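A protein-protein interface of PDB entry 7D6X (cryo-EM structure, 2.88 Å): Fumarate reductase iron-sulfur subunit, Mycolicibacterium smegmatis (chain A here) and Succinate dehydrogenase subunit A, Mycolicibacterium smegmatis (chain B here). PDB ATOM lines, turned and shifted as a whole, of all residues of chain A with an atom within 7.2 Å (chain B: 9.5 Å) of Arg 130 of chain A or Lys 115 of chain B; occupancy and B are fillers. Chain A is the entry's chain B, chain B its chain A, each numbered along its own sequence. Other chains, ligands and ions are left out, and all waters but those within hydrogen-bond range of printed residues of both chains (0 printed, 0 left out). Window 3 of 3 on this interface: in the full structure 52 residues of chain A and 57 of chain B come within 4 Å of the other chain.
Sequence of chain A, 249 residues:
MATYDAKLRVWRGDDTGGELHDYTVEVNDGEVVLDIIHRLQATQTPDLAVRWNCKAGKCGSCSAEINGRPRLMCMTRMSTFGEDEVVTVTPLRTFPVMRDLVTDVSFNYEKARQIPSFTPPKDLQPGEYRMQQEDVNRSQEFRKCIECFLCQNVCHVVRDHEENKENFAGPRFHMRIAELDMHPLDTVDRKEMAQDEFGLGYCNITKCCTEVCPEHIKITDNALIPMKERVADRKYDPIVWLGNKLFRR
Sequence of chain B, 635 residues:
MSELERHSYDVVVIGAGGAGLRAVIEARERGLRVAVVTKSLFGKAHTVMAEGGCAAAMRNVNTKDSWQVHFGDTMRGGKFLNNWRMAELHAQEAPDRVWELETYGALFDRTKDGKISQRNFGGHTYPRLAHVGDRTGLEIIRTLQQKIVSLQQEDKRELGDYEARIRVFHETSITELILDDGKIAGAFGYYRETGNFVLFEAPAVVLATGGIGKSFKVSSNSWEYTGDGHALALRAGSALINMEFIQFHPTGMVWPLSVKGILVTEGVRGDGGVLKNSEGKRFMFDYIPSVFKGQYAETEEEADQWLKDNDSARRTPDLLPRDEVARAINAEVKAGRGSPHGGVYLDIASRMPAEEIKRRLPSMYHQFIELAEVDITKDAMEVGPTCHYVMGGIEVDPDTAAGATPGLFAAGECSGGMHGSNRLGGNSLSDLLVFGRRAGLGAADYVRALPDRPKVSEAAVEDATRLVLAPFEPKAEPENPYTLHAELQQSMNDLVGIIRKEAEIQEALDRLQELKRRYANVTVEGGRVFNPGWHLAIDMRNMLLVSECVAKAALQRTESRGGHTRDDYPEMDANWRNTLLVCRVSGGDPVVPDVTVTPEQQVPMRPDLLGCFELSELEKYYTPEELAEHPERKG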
ATOM      1  N   LEU A 124     -17.751 -28.273  -5.961  1.00  0.00           N
ATOM      2  CA  LEU A 124     -17.057 -27.563  -7.021  1.00  0.00           C
ATOM      3  C   LEU A 124     -15.607 -28.015  -7.099  1.00  0.00           C
ATOM      4  O   LEU A 124     -14.963 -28.269  -6.078  1.00  0.00           O
ATOM      5  CB  LEU A 124     -17.141 -26.062  -6.758  1.00  0.00           C
ATOM      6  CG  LEU A 124     -16.884 -25.068  -7.879  1.00  0.00           C
ATOM      7  CD1 LEU A 124     -17.912 -25.266  -8.965  1.00  0.00           C
ATOM      8  CD2 LEU A 124     -16.971 -23.667  -7.333  1.00  0.00           C
ATOM      9  N   PRO A 126     -11.509 -27.511  -8.495  1.00  0.00           N
ATOM     10  CA  PRO A 126     -10.620 -26.336  -8.501  1.00  0.00           C
ATOM     11  C   PRO A 126     -10.561 -25.595  -9.826  1.00  0.00           C
ATOM     12  O   PRO A 126     -10.490 -24.360  -9.828  1.00  0.00           O
ATOM     13  CB  PRO A 126      -9.256 -26.928  -8.112  1.00  0.00           C
ATOM     14  CG  PRO A 126      -9.392 -28.394  -8.277  1.00  0.00           C
ATOM     15  CD  PRO A 126     -10.815 -28.711  -8.004  1.00  0.00           C
ATOM     16  N   GLY A 127     -10.589 -26.296 -10.950  1.00  0.00           N
ATOM     17  CA  GLY A 127     -10.537 -25.603 -12.218  1.00  0.00           C
ATOM     18  C   GLY A 127     -11.849 -25.045 -12.718  1.00  0.00           C
ATOM     19  O   GLY A 127     -11.917 -24.595 -13.864  1.00  0.00           O
ATOM     20  N   GLU A 128     -12.897 -25.048 -11.892  1.00  0.00           N
ATOM     21  CA  GLU A 128     -14.249 -24.726 -12.327  1.00  0.00           C
ATOM     22  C   GLU A 128     -14.861 -23.580 -11.528  1.00  0.00           C
ATOM     23  O   GLU A 128     -16.079 -23.506 -11.381  1.00  0.00           O
ATOM     24  CB  GLU A 128     -15.142 -25.961 -12.242  1.00  0.00           C
ATOM     25  N   TYR A 129     -14.034 -22.676 -11.014  1.00  0.00           N
ATOM     26  CA  TYR A 129     -14.513 -21.500 -10.302  1.00  0.00           C
ATOM     27  C   TYR A 129     -14.725 -20.372 -11.302  1.00  0.00           C
ATOM     28  O   TYR A 129     -13.785 -19.973 -11.997  1.00  0.00           O
ATOM     29  CB  TYR A 129     -13.518 -21.067  -9.227  1.00  0.00           C
ATOM     30  CG  TYR A 129     -13.537 -21.891  -7.960  1.00  0.00           C
ATOM     31  CD1 TYR A 129     -13.508 -23.273  -8.005  1.00  0.00           C
ATOM     32  CD2 TYR A 129     -13.558 -21.284  -6.718  1.00  0.00           C
ATOM     33  CE1 TYR A 129     -13.516 -24.023  -6.855  1.00  0.00           C
ATOM     34  CE2 TYR A 129     -13.569 -22.025  -5.562  1.00  0.00           C
ATOM     35  CZ  TYR A 129     -13.548 -23.397  -5.636  1.00  0.00           C
ATOM     36  OH  TYR A 129     -13.556 -24.153  -4.490  1.00  0.00           O
ATOM     37  N   ARG A 130     -15.949 -19.856 -11.376  1.00  0.00           N
ATOM     38  CA  ARG A 130     -16.294 -18.779 -12.296  1.00  0.00           C
ATOM     39  C   ARG A 130     -16.835 -17.601 -11.506  1.00  0.00           C
ATOM     40  O   ARG A 130     -17.885 -17.711 -10.867  1.00  0.00           O
ATOM     41  CB  ARG A 130     -17.323 -19.236 -13.326  1.00  0.00           C
ATOM     42  CG  ARG A 130     -16.876 -20.399 -14.169  1.00  0.00           C
ATOM     43  CD  ARG A 130     -15.836 -19.990 -15.185  1.00  0.00           C
ATOM     44  NE  ARG A 130     -15.420 -21.130 -15.988  1.00  0.00           N
ATOM     45  CZ  ARG A 130     -14.299 -21.809 -15.794  1.00  0.00           C
ATOM     46  NH1 ARG A 130     -13.468 -21.462 -14.827  1.00  0.00           N
ATOM     47  NH2 ARG A 130     -14.006 -22.839 -16.571  1.00  0.00           N
ATOM     48  N   MET A 131     -16.128 -16.480 -11.556  1.00  0.00           N
ATOM     49  CA  MET A 131     -16.555 -15.260 -10.892  1.00  0.00           C
ATOM     50  C   MET A 131     -16.360 -14.092 -11.841  1.00  0.00           C
ATOM     51  O   MET A 131     -15.357 -14.028 -12.552  1.00  0.00           O
ATOM     52  CB  MET A 131     -15.766 -15.023  -9.605  1.00  0.00           C
ATOM     53  CG  MET A 131     -15.992 -16.073  -8.543  1.00  0.00           C
ATOM     54  SD  MET A 131     -14.875 -15.916  -7.147  1.00  0.00           S
ATOM     55  CE  MET A 131     -13.541 -16.971  -7.672  1.00  0.00           C
ATOM     56  N   GLN A 132     -17.315 -13.174 -11.855  1.00  0.00           N
ATOM     57  CA  GLN A 132     -17.182 -11.978 -12.668  1.00  0.00           C
ATOM     58  C   GLN A 132     -16.431 -10.902 -11.896  1.00  0.00           C
ATOM     59  O   GLN A 132     -16.366 -10.917 -10.668  1.00  0.00           O
ATOM     60  CB  GLN A 132     -18.550 -11.465 -13.102  1.00  0.00           C
ATOM     61  CG  GLN A 132     -19.368 -12.488 -13.849  1.00  0.00           C
ATOM     62  CD  GLN A 132     -18.719 -12.917 -15.140  1.00  0.00           C
ATOM     63  OE1 GLN A 132     -18.154 -12.101 -15.863  1.00  0.00           O
ATOM     64  NE2 GLN A 132     -18.794 -14.205 -15.439  1.00  0.00           N
ATOM     65  N   ASP A 135     -18.139  -8.905  -9.239  1.00  0.00           N
ATOM     66  CA  ASP A 135     -18.421  -9.643  -8.014  1.00  0.00           C
ATOM     67  C   ASP A 135     -17.215  -9.668  -7.085  1.00  0.00           C
ATOM     68  O   ASP A 135     -17.372  -9.632  -5.861  1.00  0.00           O
ATOM     69  CB  ASP A 135     -18.858 -11.065  -8.348  1.00  0.00           C
ATOM     70  CG  ASP A 135     -20.095 -11.103  -9.205  1.00  0.00           C
ATOM     71  OD1 ASP A 135     -20.535 -10.026  -9.642  1.00  0.00           O
ATOM     72  OD2 ASP A 135     -20.628 -12.204  -9.443  1.00  0.00           O
ATOM     73  N   VAL A 136     -16.006  -9.726  -7.644  1.00  0.00           N
ATOM     74  CA  VAL A 136     -14.798  -9.781  -6.829  1.00  0.00           C
ATOM     75  C   VAL A 136     -14.246  -8.405  -6.500  1.00  0.00           C
ATOM     76  O   VAL A 136     -13.314  -8.306  -5.687  1.00  0.00           O
ATOM     77  CB  VAL A 136     -13.702 -10.606  -7.529  1.00  0.00           C
ATOM     78  CG1 VAL A 136     -14.256 -11.935  -7.984  1.00  0.00           C
ATOM     79  CG2 VAL A 136     -13.137  -9.848  -8.701  1.00  0.00           C
ATOM     80  N   PRO A 184     -18.151 -13.882  -3.544  1.00  0.00           N
ATOM     81  CA  PRO A 184     -19.280 -14.427  -4.312  1.00  0.00           C
ATOM     82  C   PRO A 184     -19.461 -15.926  -4.183  1.00  0.00           C
ATOM     83  O   PRO A 184     -20.513 -16.436  -4.582  1.00  0.00           O
ATOM     84  CB  PRO A 184     -18.942 -14.030  -5.753  1.00  0.00           C
ATOM     85  CG  PRO A 184     -17.479 -13.831  -5.756  1.00  0.00           C
ATOM     86  CD  PRO A 184     -17.131 -13.282  -4.418  1.00  0.00           C
ATOM     87  N   LEU A 185     -18.490 -16.655  -3.640  1.00  0.00           N
ATOM     88  CA  LEU A 185     -18.561 -18.107  -3.583  1.00  0.00           C
ATOM     89  C   LEU A 185     -18.566 -18.668  -2.168  1.00  0.00           C
ATOM     90  O   LEU A 185     -18.621 -19.890  -2.008  1.00  0.00           O
ATOM     91  CB  LEU A 185     -17.400 -18.717  -4.373  1.00  0.00           C
ATOM     92  CG  LEU A 185     -17.671 -18.936  -5.859  1.00  0.00           C
ATOM     93  CD1 LEU A 185     -16.390 -19.221  -6.589  1.00  0.00           C
ATOM     94  CD2 LEU A 185     -18.647 -20.071  -6.054  1.00  0.00           C
ATOM     95  N   MET B  58      -2.532 -22.035 -18.223  1.00  0.00           N
ATOM     96  CA  MET B  58      -3.941 -22.317 -17.998  1.00  0.00           C
ATOM     97  C   MET B  58      -4.785 -22.176 -19.254  1.00  0.00           C
ATOM     98  O   MET B  58      -5.902 -22.700 -19.285  1.00  0.00           O
ATOM     99  CB  MET B  58      -4.487 -21.397 -16.911  1.00  0.00           C
ATOM    100  CG  MET B  58      -4.041 -21.778 -15.523  1.00  0.00           C
ATOM    101  SD  MET B  58      -4.767 -20.762 -14.238  1.00  0.00           S
ATOM    102  CE  MET B  58      -3.797 -19.281 -14.417  1.00  0.00           C
ATOM    103  N   ARG B  59      -4.282 -21.483 -20.276  1.00  0.00           N
ATOM    104  CA  ARG B  59      -4.980 -21.308 -21.550  1.00  0.00           C
ATOM    105  C   ARG B  59      -6.306 -20.578 -21.369  1.00  0.00           C
ATOM    106  O   ARG B  59      -7.309 -20.909 -22.002  1.00  0.00           O
ATOM    107  CB  ARG B  59      -5.184 -22.649 -22.252  1.00  0.00           C
ATOM    108  CG  ARG B  59      -3.916 -23.443 -22.415  1.00  0.00           C
ATOM    109  CD  ARG B  59      -4.203 -24.915 -22.557  1.00  0.00           C
ATOM    110  NE  ARG B  59      -4.442 -25.285 -23.943  1.00  0.00           N
ATOM    111  CZ  ARG B  59      -5.645 -25.460 -24.470  1.00  0.00           C
ATOM    112  NH1 ARG B  59      -6.728 -25.294 -23.725  1.00  0.00           N
ATOM    113  NH2 ARG B  59      -5.766 -25.799 -25.745  1.00  0.00           N
ATOM    114  N   ASN B  60      -6.312 -19.566 -20.501  1.00  0.00           N
ATOM    115  CA  ASN B  60      -7.521 -18.780 -20.289  1.00  0.00           C
ATOM    116  C   ASN B  60      -7.671 -17.691 -21.341  1.00  0.00           C
ATOM    117  O   ASN B  60      -8.779 -17.445 -21.825  1.00  0.00           O
ATOM    118  CB  ASN B  60      -7.516 -18.162 -18.892  1.00  0.00           C
ATOM    119  CG  ASN B  60      -7.640 -19.194 -17.799  1.00  0.00           C
ATOM    120  OD1 ASN B  60      -8.063 -20.320 -18.037  1.00  0.00           O
ATOM    121  ND2 ASN B  60      -7.275 -18.812 -16.587  1.00  0.00           N
ATOM    122  N   VAL B  61      -6.575 -17.030 -21.707  1.00  0.00           N
ATOM    123  CA  VAL B  61      -6.648 -15.959 -22.694  1.00  0.00           C
ATOM    124  C   VAL B  61      -6.660 -16.528 -24.106  1.00  0.00           C
ATOM    125  O   VAL B  61      -7.634 -16.368 -24.849  1.00  0.00           O
ATOM    126  CB  VAL B  61      -5.492 -14.965 -22.496  1.00  0.00           C
ATOM    127  CG1 VAL B  61      -5.549 -13.886 -23.549  1.00  0.00           C
ATOM    128  CG2 VAL B  61      -5.566 -14.353 -21.119  1.00  0.00           C
ATOM    129  N   ASN B  62      -5.588 -17.210 -24.498  1.00  0.00           N
ATOM    130  CA  ASN B  62      -5.549 -17.881 -25.789  1.00  0.00           C
ATOM    131  C   ASN B  62      -5.207 -19.347 -25.582  1.00  0.00           C
ATOM    132  O   ASN B  62      -4.350 -19.688 -24.765  1.00  0.00           O
ATOM    133  CB  ASN B  62      -4.553 -17.219 -26.757  1.00  0.00           C
ATOM    134  CG  ASN B  62      -3.114 -17.463 -26.383  1.00  0.00           C
ATOM    135  OD1 ASN B  62      -2.762 -17.496 -25.207  1.00  0.00           O
ATOM    136  ND2 ASN B  62      -2.267 -17.627 -27.388  1.00  0.00           N
ATOM    137  N   THR B  63      -5.892 -20.206 -26.325  1.00  0.00           N
ATOM    138  CA  THR B  63      -5.850 -21.642 -26.105  1.00  0.00           C
ATOM    139  C   THR B  63      -4.727 -22.335 -26.853  1.00  0.00           C
ATOM    140  O   THR B  63      -4.617 -23.561 -26.768  1.00  0.00           O
ATOM    141  CB  THR B  63      -7.182 -22.271 -26.506  1.00  0.00           C
ATOM    142  OG1 THR B  63      -7.340 -22.184 -27.925  1.00  0.00           O
ATOM    143  CG2 THR B  63      -8.325 -21.547 -25.833  1.00  0.00           C
ATOM    144  N   VAL B  98      -2.102 -23.005  -9.266  1.00  0.00           N
ATOM    145  CA  VAL B  98      -2.827 -21.742  -9.298  1.00  0.00           C
ATOM    146  C   VAL B  98      -4.326 -21.987  -9.206  1.00  0.00           C
ATOM    147  O   VAL B  98      -5.059 -21.200  -8.597  1.00  0.00           O
ATOM    148  CB  VAL B  98      -2.460 -20.952 -10.564  1.00  0.00           C
ATOM    149  CG1 VAL B  98      -2.996 -19.544 -10.474  1.00  0.00           C
ATOM    150  CG2 VAL B  98      -0.961 -20.935 -10.751  1.00  0.00           C
ATOM    151  N   TRP B  99      -4.807 -23.078  -9.798  1.00  0.00           N
ATOM    152  CA  TRP B  99      -6.234 -23.373  -9.737  1.00  0.00           C
ATOM    153  C   TRP B  99      -6.665 -23.747  -8.330  1.00  0.00           C
ATOM    154  O   TRP B  99      -7.782 -23.428  -7.916  1.00  0.00           O
ATOM    155  CB  TRP B  99      -6.583 -24.491 -10.709  1.00  0.00           C
ATOM    156  CG  TRP B  99      -6.932 -23.991 -12.047  1.00  0.00           C
ATOM    157  CD1 TRP B  99      -7.455 -22.777 -12.351  1.00  0.00           C
ATOM    158  CD2 TRP B  99      -6.779 -24.686 -13.281  1.00  0.00           C
ATOM    159  NE1 TRP B  99      -7.642 -22.669 -13.703  1.00  0.00           N
ATOM    160  CE2 TRP B  99      -7.231 -23.831 -14.297  1.00  0.00           C
ATOM    161  CE3 TRP B  99      -6.303 -25.951 -13.627  1.00  0.00           C
ATOM    162  CZ2 TRP B  99      -7.225 -24.198 -15.631  1.00  0.00           C
ATOM    163  CZ3 TRP B  99      -6.296 -26.311 -14.950  1.00  0.00           C
ATOM    164  CH2 TRP B  99      -6.753 -25.440 -15.938  1.00  0.00           C
ATOM    165  N   GLU B 102      -7.183 -20.698  -5.712  1.00  0.00           N
ATOM    166  CA  GLU B 102      -8.464 -20.014  -5.639  1.00  0.00           C
ATOM    167  C   GLU B 102      -9.533 -20.828  -4.930  1.00  0.00           C
ATOM    168  O   GLU B 102     -10.621 -20.300  -4.684  1.00  0.00           O
ATOM    169  CB  GLU B 102      -8.943 -19.639  -7.038  1.00  0.00           C
ATOM    170  CG  GLU B 102      -9.414 -20.799  -7.869  1.00  0.00           C
ATOM    171  CD  GLU B 102      -9.948 -20.358  -9.209  1.00  0.00           C
ATOM    172  OE1 GLU B 102     -10.204 -19.150  -9.372  1.00  0.00           O
ATOM    173  OE2 GLU B 102     -10.112 -21.215 -10.101  1.00  0.00           O
ATOM    174  N   LEU B 107      -8.500 -14.334  -4.794  1.00  0.00           N
ATOM    175  CA  LEU B 107      -9.312 -13.586  -5.753  1.00  0.00           C
ATOM    176  C   LEU B 107      -8.377 -12.889  -6.733  1.00  0.00           C
ATOM    177  O   LEU B 107      -7.861 -11.809  -6.441  1.00  0.00           O
ATOM    178  CB  LEU B 107     -10.209 -12.576  -5.049  1.00  0.00           C
ATOM    179  CG  LEU B 107     -11.315 -13.123  -4.155  1.00  0.00           C
ATOM    180  CD1 LEU B 107     -11.662 -12.099  -3.111  1.00  0.00           C
ATOM    181  CD2 LEU B 107     -12.531 -13.472  -4.976  1.00  0.00           C
ATOM    182  N   PHE B 108      -8.162 -13.505  -7.888  1.00  0.00           N
ATOM    183  CA  PHE B 108      -7.359 -12.890  -8.928  1.00  0.00           C
ATOM    184  C   PHE B 108      -8.222 -11.950  -9.762  1.00  0.00           C
ATOM    185  O   PHE B 108      -9.411 -11.757  -9.502  1.00  0.00           O
ATOM    186  CB  PHE B 108      -6.723 -13.955  -9.813  1.00  0.00           C
ATOM    187  CG  PHE B 108      -5.758 -14.843  -9.097  1.00  0.00           C
ATOM    188  CD1 PHE B 108      -4.446 -14.456  -8.915  1.00  0.00           C
ATOM    189  CD2 PHE B 108      -6.157 -16.072  -8.618  1.00  0.00           C
ATOM    190  CE1 PHE B 108      -3.560 -15.270  -8.265  1.00  0.00           C
ATOM    191  CE2 PHE B 108      -5.273 -16.891  -7.967  1.00  0.00           C
ATOM    192  CZ  PHE B 108      -3.973 -16.490  -7.790  1.00  0.00           C
ATOM    193  N   ASP B 109      -7.616 -11.353 -10.779  1.00  0.00           N
ATOM    194  CA  ASP B 109      -8.383 -10.583 -11.742  1.00  0.00           C
ATOM    195  C   ASP B 109      -9.071 -11.528 -12.714  1.00  0.00           C
ATOM    196  O   ASP B 109      -8.522 -12.564 -13.090  1.00  0.00           O
ATOM    197  CB  ASP B 109      -7.480  -9.605 -12.482  1.00  0.00           C
ATOM    198  CG  ASP B 109      -7.247  -8.330 -11.701  1.00  0.00           C
ATOM    199  OD1 ASP B 109      -7.511  -8.327 -10.482  1.00  0.00           O
ATOM    200  OD2 ASP B 109      -6.805  -7.330 -12.299  1.00  0.00           O
ATOM    201  N   ARG B 110     -10.282 -11.171 -13.115  1.00  0.00           N
ATOM    202  CA  ARG B 110     -11.147 -12.059 -13.869  1.00  0.00           C
ATOM    203  C   ARG B 110     -11.269 -11.589 -15.308  1.00  0.00           C
ATOM    204  O   ARG B 110     -11.123 -10.402 -15.605  1.00  0.00           O
ATOM    205  CB  ARG B 110     -12.525 -12.131 -13.213  1.00  0.00           C
ATOM    206  CG  ARG B 110     -12.469 -12.745 -11.842  1.00  0.00           C
ATOM    207  CD  ARG B 110     -12.281 -14.224 -11.981  1.00  0.00           C
ATOM    208  NE  ARG B 110     -11.698 -14.845 -10.807  1.00  0.00           N
ATOM    209  CZ  ARG B 110     -11.511 -16.150 -10.695  1.00  0.00           C
ATOM    210  NH1 ARG B 110     -11.893 -16.953 -11.671  1.00  0.00           N
ATOM    211  NH2 ARG B 110     -10.960 -16.652  -9.604  1.00  0.00           N
ATOM    212  N   THR B 111     -11.524 -12.535 -16.203  1.00  0.00           N
ATOM    213  CA  THR B 111     -11.769 -12.221 -17.599  1.00  0.00           C
ATOM    214  C   THR B 111     -13.247 -11.894 -17.793  1.00  0.00           C
ATOM    215  O   THR B 111     -14.015 -11.796 -16.832  1.00  0.00           O
ATOM    216  CB  THR B 111     -11.333 -13.378 -18.491  1.00  0.00           C
ATOM    217  OG1 THR B 111     -12.317 -14.412 -18.451  1.00  0.00           O
ATOM    218  CG2 THR B 111     -10.016 -13.935 -18.029  1.00  0.00           C
ATOM    219  N   LYS B 112     -13.669 -11.723 -19.044  1.00  0.00           N
ATOM    220  CA  LYS B 112     -15.086 -11.573 -19.331  1.00  0.00           C
ATOM    221  C   LYS B 112     -15.840 -12.888 -19.236  1.00  0.00           C
ATOM    222  O   LYS B 112     -17.069 -12.889 -19.354  1.00  0.00           O
ATOM    223  CB  LYS B 112     -15.295 -10.984 -20.725  1.00  0.00           C
ATOM    224  CG  LYS B 112     -14.684  -9.616 -20.926  1.00  0.00           C
ATOM    225  CD  LYS B 112     -15.360  -8.569 -20.065  1.00  0.00           C
ATOM    226  CE  LYS B 112     -14.858  -7.182 -20.425  1.00  0.00           C
ATOM    227  NZ  LYS B 112     -13.425  -7.006 -20.063  1.00  0.00           N
ATOM    228  N   ASP B 113     -15.140 -14.001 -19.037  1.00  0.00           N
ATOM    229  CA  ASP B 113     -15.774 -15.304 -18.931  1.00  0.00           C
ATOM    230  C   ASP B 113     -15.833 -15.807 -17.497  1.00  0.00           C
ATOM    231  O   ASP B 113     -16.571 -16.755 -17.212  1.00  0.00           O
ATOM    232  CB  ASP B 113     -15.023 -16.315 -19.800  1.00  0.00           C
ATOM    233  CG  ASP B 113     -15.857 -17.527 -20.147  1.00  0.00           C
ATOM    234  OD1 ASP B 113     -15.403 -18.330 -20.986  1.00  0.00           O
ATOM    235  OD2 ASP B 113     -16.973 -17.674 -19.608  1.00  0.00           O
ATOM    236  N   GLY B 114     -15.084 -15.193 -16.590  1.00  0.00           N
ATOM    237  CA  GLY B 114     -15.023 -15.631 -15.219  1.00  0.00           C
ATOM    238  C   GLY B 114     -13.751 -16.356 -14.850  1.00  0.00           C
ATOM    239  O   GLY B 114     -13.540 -16.638 -13.667  1.00  0.00           O
ATOM    240  N   LYS B 115     -12.903 -16.665 -15.822  1.00  0.00           N
ATOM    241  CA  LYS B 115     -11.646 -17.336 -15.556  1.00  0.00           C
ATOM    242  C   LYS B 115     -10.598 -16.339 -15.076  1.00  0.00           C
ATOM    243  O   LYS B 115     -10.804 -15.128 -15.080  1.00  0.00           O
ATOM    244  CB  LYS B 115     -11.163 -18.060 -16.805  1.00  0.00           C
ATOM    245  CG  LYS B 115     -12.265 -18.726 -17.576  1.00  0.00           C
ATOM    246  CD  LYS B 115     -11.710 -19.675 -18.606  1.00  0.00           C
ATOM    247  CE  LYS B 115     -12.808 -20.507 -19.221  1.00  0.00           C
ATOM    248  NZ  LYS B 115     -12.262 -21.597 -20.059  1.00  0.00           N
ATOM    249  N   ILE B 116      -9.453 -16.870 -14.652  1.00  0.00           N
ATOM    250  CA  ILE B 116      -8.375 -16.030 -14.147  1.00  0.00           C
ATOM    251  C   ILE B 116      -7.704 -15.302 -15.304  1.00  0.00           C
ATOM    252  O   ILE B 116      -7.412 -15.894 -16.351  1.00  0.00           O
ATOM    253  CB  ILE B 116      -7.361 -16.879 -13.363  1.00  0.00           C
ATOM    254  CG1 ILE B 116      -8.054 -17.611 -12.221  1.00  0.00           C
ATOM    255  CG2 ILE B 116      -6.252 -16.016 -12.820  1.00  0.00           C
ATOM    256  CD1 ILE B 116      -7.116 -18.416 -11.365  1.00  0.00           C
ATOM    257  N   SER B 117      -7.455 -14.010 -15.118  1.00  0.00           N
ATOM    258  CA  SER B 117      -6.874 -13.190 -16.168  1.00  0.00           C
ATOM    259  C   SER B 117      -5.362 -13.337 -16.182  1.00  0.00           C
ATOM    260  O   SER B 117      -4.726 -13.453 -15.134  1.00  0.00           O
ATOM    261  CB  SER B 117      -7.252 -11.726 -15.971  1.00  0.00           C
ATOM    262  OG  SER B 117      -6.661 -10.914 -16.964  1.00  0.00           O
ATOM    263  N   GLN B 118      -4.786 -13.316 -17.380  1.00  0.00           N
ATOM    264  CA  GLN B 118      -3.367 -13.564 -17.575  1.00  0.00           C
ATOM    265  C   GLN B 118      -2.732 -12.426 -18.361  1.00  0.00           C
ATOM    266  O   GLN B 118      -3.310 -11.930 -19.332  1.00  0.00           O
ATOM    267  CB  GLN B 118      -3.158 -14.888 -18.292  1.00  0.00           C
ATOM    268  CG  GLN B 118      -3.708 -16.063 -17.523  1.00  0.00           C
ATOM    269  CD  GLN B 118      -3.531 -17.368 -18.245  1.00  0.00           C
ATOM    270  OE1 GLN B 118      -3.839 -17.487 -19.425  1.00  0.00           O
ATOM    271  NE2 GLN B 118      -3.020 -18.359 -17.541  1.00  0.00           N
ATOM    272  N   ALA B 130      -0.795 -15.117 -14.255  1.00  0.00           N
ATOM    273  CA  ALA B 130      -2.009 -14.850 -13.497  1.00  0.00           C
ATOM    274  C   ALA B 130      -1.724 -13.821 -12.417  1.00  0.00           C
ATOM    275  O   ALA B 130      -0.772 -13.964 -11.649  1.00  0.00           O
ATOM    276  CB  ALA B 130      -2.536 -16.139 -12.875  1.00  0.00           C
ATOM    277  N   HIS B 131      -2.555 -12.787 -12.344  1.00  0.00           N
ATOM    278  CA  HIS B 131      -2.247 -11.628 -11.523  1.00  0.00           C
ATOM    279  C   HIS B 131      -3.497 -11.120 -10.824  1.00  0.00           C
ATOM    280  O   HIS B 131      -4.621 -11.492 -11.159  1.00  0.00           O
ATOM    281  CB  HIS B 131      -1.652 -10.503 -12.369  1.00  0.00           C
ATOM    282  CG  HIS B 131      -2.612  -9.935 -13.364  1.00  0.00           C
ATOM    283  ND1 HIS B 131      -3.238  -8.722 -13.186  1.00  0.00           N
ATOM    284  CD2 HIS B 131      -3.065 -10.422 -14.542  1.00  0.00           C
ATOM    285  CE1 HIS B 131      -4.029  -8.482 -14.214  1.00  0.00           C
ATOM    286  NE2 HIS B 131      -3.943  -9.499 -15.051  1.00  0.00           N
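The backbone carbonyl oxygen (O) of Gly 114 of chain B lies within hydrogen-bond range of the backbone NH (N) of Met 131 of chain A (3.3 Å).
O of Pro 126 of chain A sits close to O of Trp 99 of chain B, 3.4 Å away.
The backbone carbonyl oxygen (O) of Pro 126 of chain A lies close to the side-chain carboxylate (OE2) of Glu 102 of chain B (3.2 Å).
Printed residues of chain B within 4 Å of Pro 126 of chain A: Trp 99 and Glu 102.
Of chain B, only Asp 113 (3.9 Å), Gly 114 (3.7 Å) and Lys 115 (3.7 Å) come within 4 Å of Arg 130 of chain A.
Printed residues of chain A within 4 Å of Leu 107 of chain B: Val 136 (3.8 Å).
Phe 108 of chain B touches none of the printed residues of chain A.
Of the printed residues of chain A, Lys 112 of chain B touches Gln 132.
Of the printed residues of chain A, Gly 114 of chain B touches Tyr 129, Arg 130 and Met 131.
Lys 115 of chain B touches just one residue of chain A: Arg 130.
The nearest residue of chain B that does not touch Arg 130 of chain A is Arg 110 of chain B (4.8 Å).
The nearest residue of chain A that does not touch Lys 115 of chain B is Met 131 of chain A (4.9 Å).
The nearest printed residue of chain A that does not touch Leu 107 of chain B is Met 131 of chain A (4.02 Å).
Among the printed residues, pairs that only touch across the chains: Gly 127 of chain A with Trp 99 of chain B (3.95 Å), Tyr 129 of chain A with Glu 102 of chain B (3.5 Å), Tyr 129 of chain A with Arg 110 of chain B (3.6 Å), Tyr 129 of chain A with Gly 114 of chain B (3.7 Å), Arg 130 of chain A with Asp 113 of chain B (3.9 Å), Arg 130 of chain A with Gly 114 of chain B (3.7 Å), Arg 130 of chain A with Lys 115 of chain B (3.7 Å), Met 131 of chain A with Arg 110 of chain B (3.1 Å), Gln 132 of chain A with Lys 112 of chain B (3.7 Å), Gln 132 of chain A with Asp 113 of chain B (3.8 Å) and Val 136 of chain A with Leu 107 of chain B (3.8 Å).
The indole nitrogen of Trp 99 of chain B sits at hydrogen-bond distance from the side-chain sulfur of Met 58 of chain B (3.5 Å).
The side-chain hydroxyl (OG1) of Thr 111 of chain B sits at hydrogen-bond distance from the backbone NH (N) of Asp 113 of chain B.
The side-chain hydroxyl (OG1) of Thr 111 of chain B is in hydrogen-bond range of the backbone NH (N) of Gly 114 of chain B.
Of the 12 printed residues of chain A, 7 touch a printed residue of chain B.
Hydrophobic or aromatic side chains of chain A within 4 Å of the printed part of chain B: Pro 126, Tyr 129, Met 131 and Val 136.
Printed residues of chain B that touch a printed residue of chain A: Trp 99, Glu 102, Leu 107, Arg 110, Lys 112, Asp 113, Gly 114 and Lys 115.
Hydrophobic or aromatic side chains of chain B that line the printed part of chain A: Trp 99 and Leu 107.
Among the printed residues, 14 pairs touch across the chains.
Among the printed residues, no Asp or Glu carboxylate lies within 4 Å of a Lys or Arg side-chain nitrogen of the other chain.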
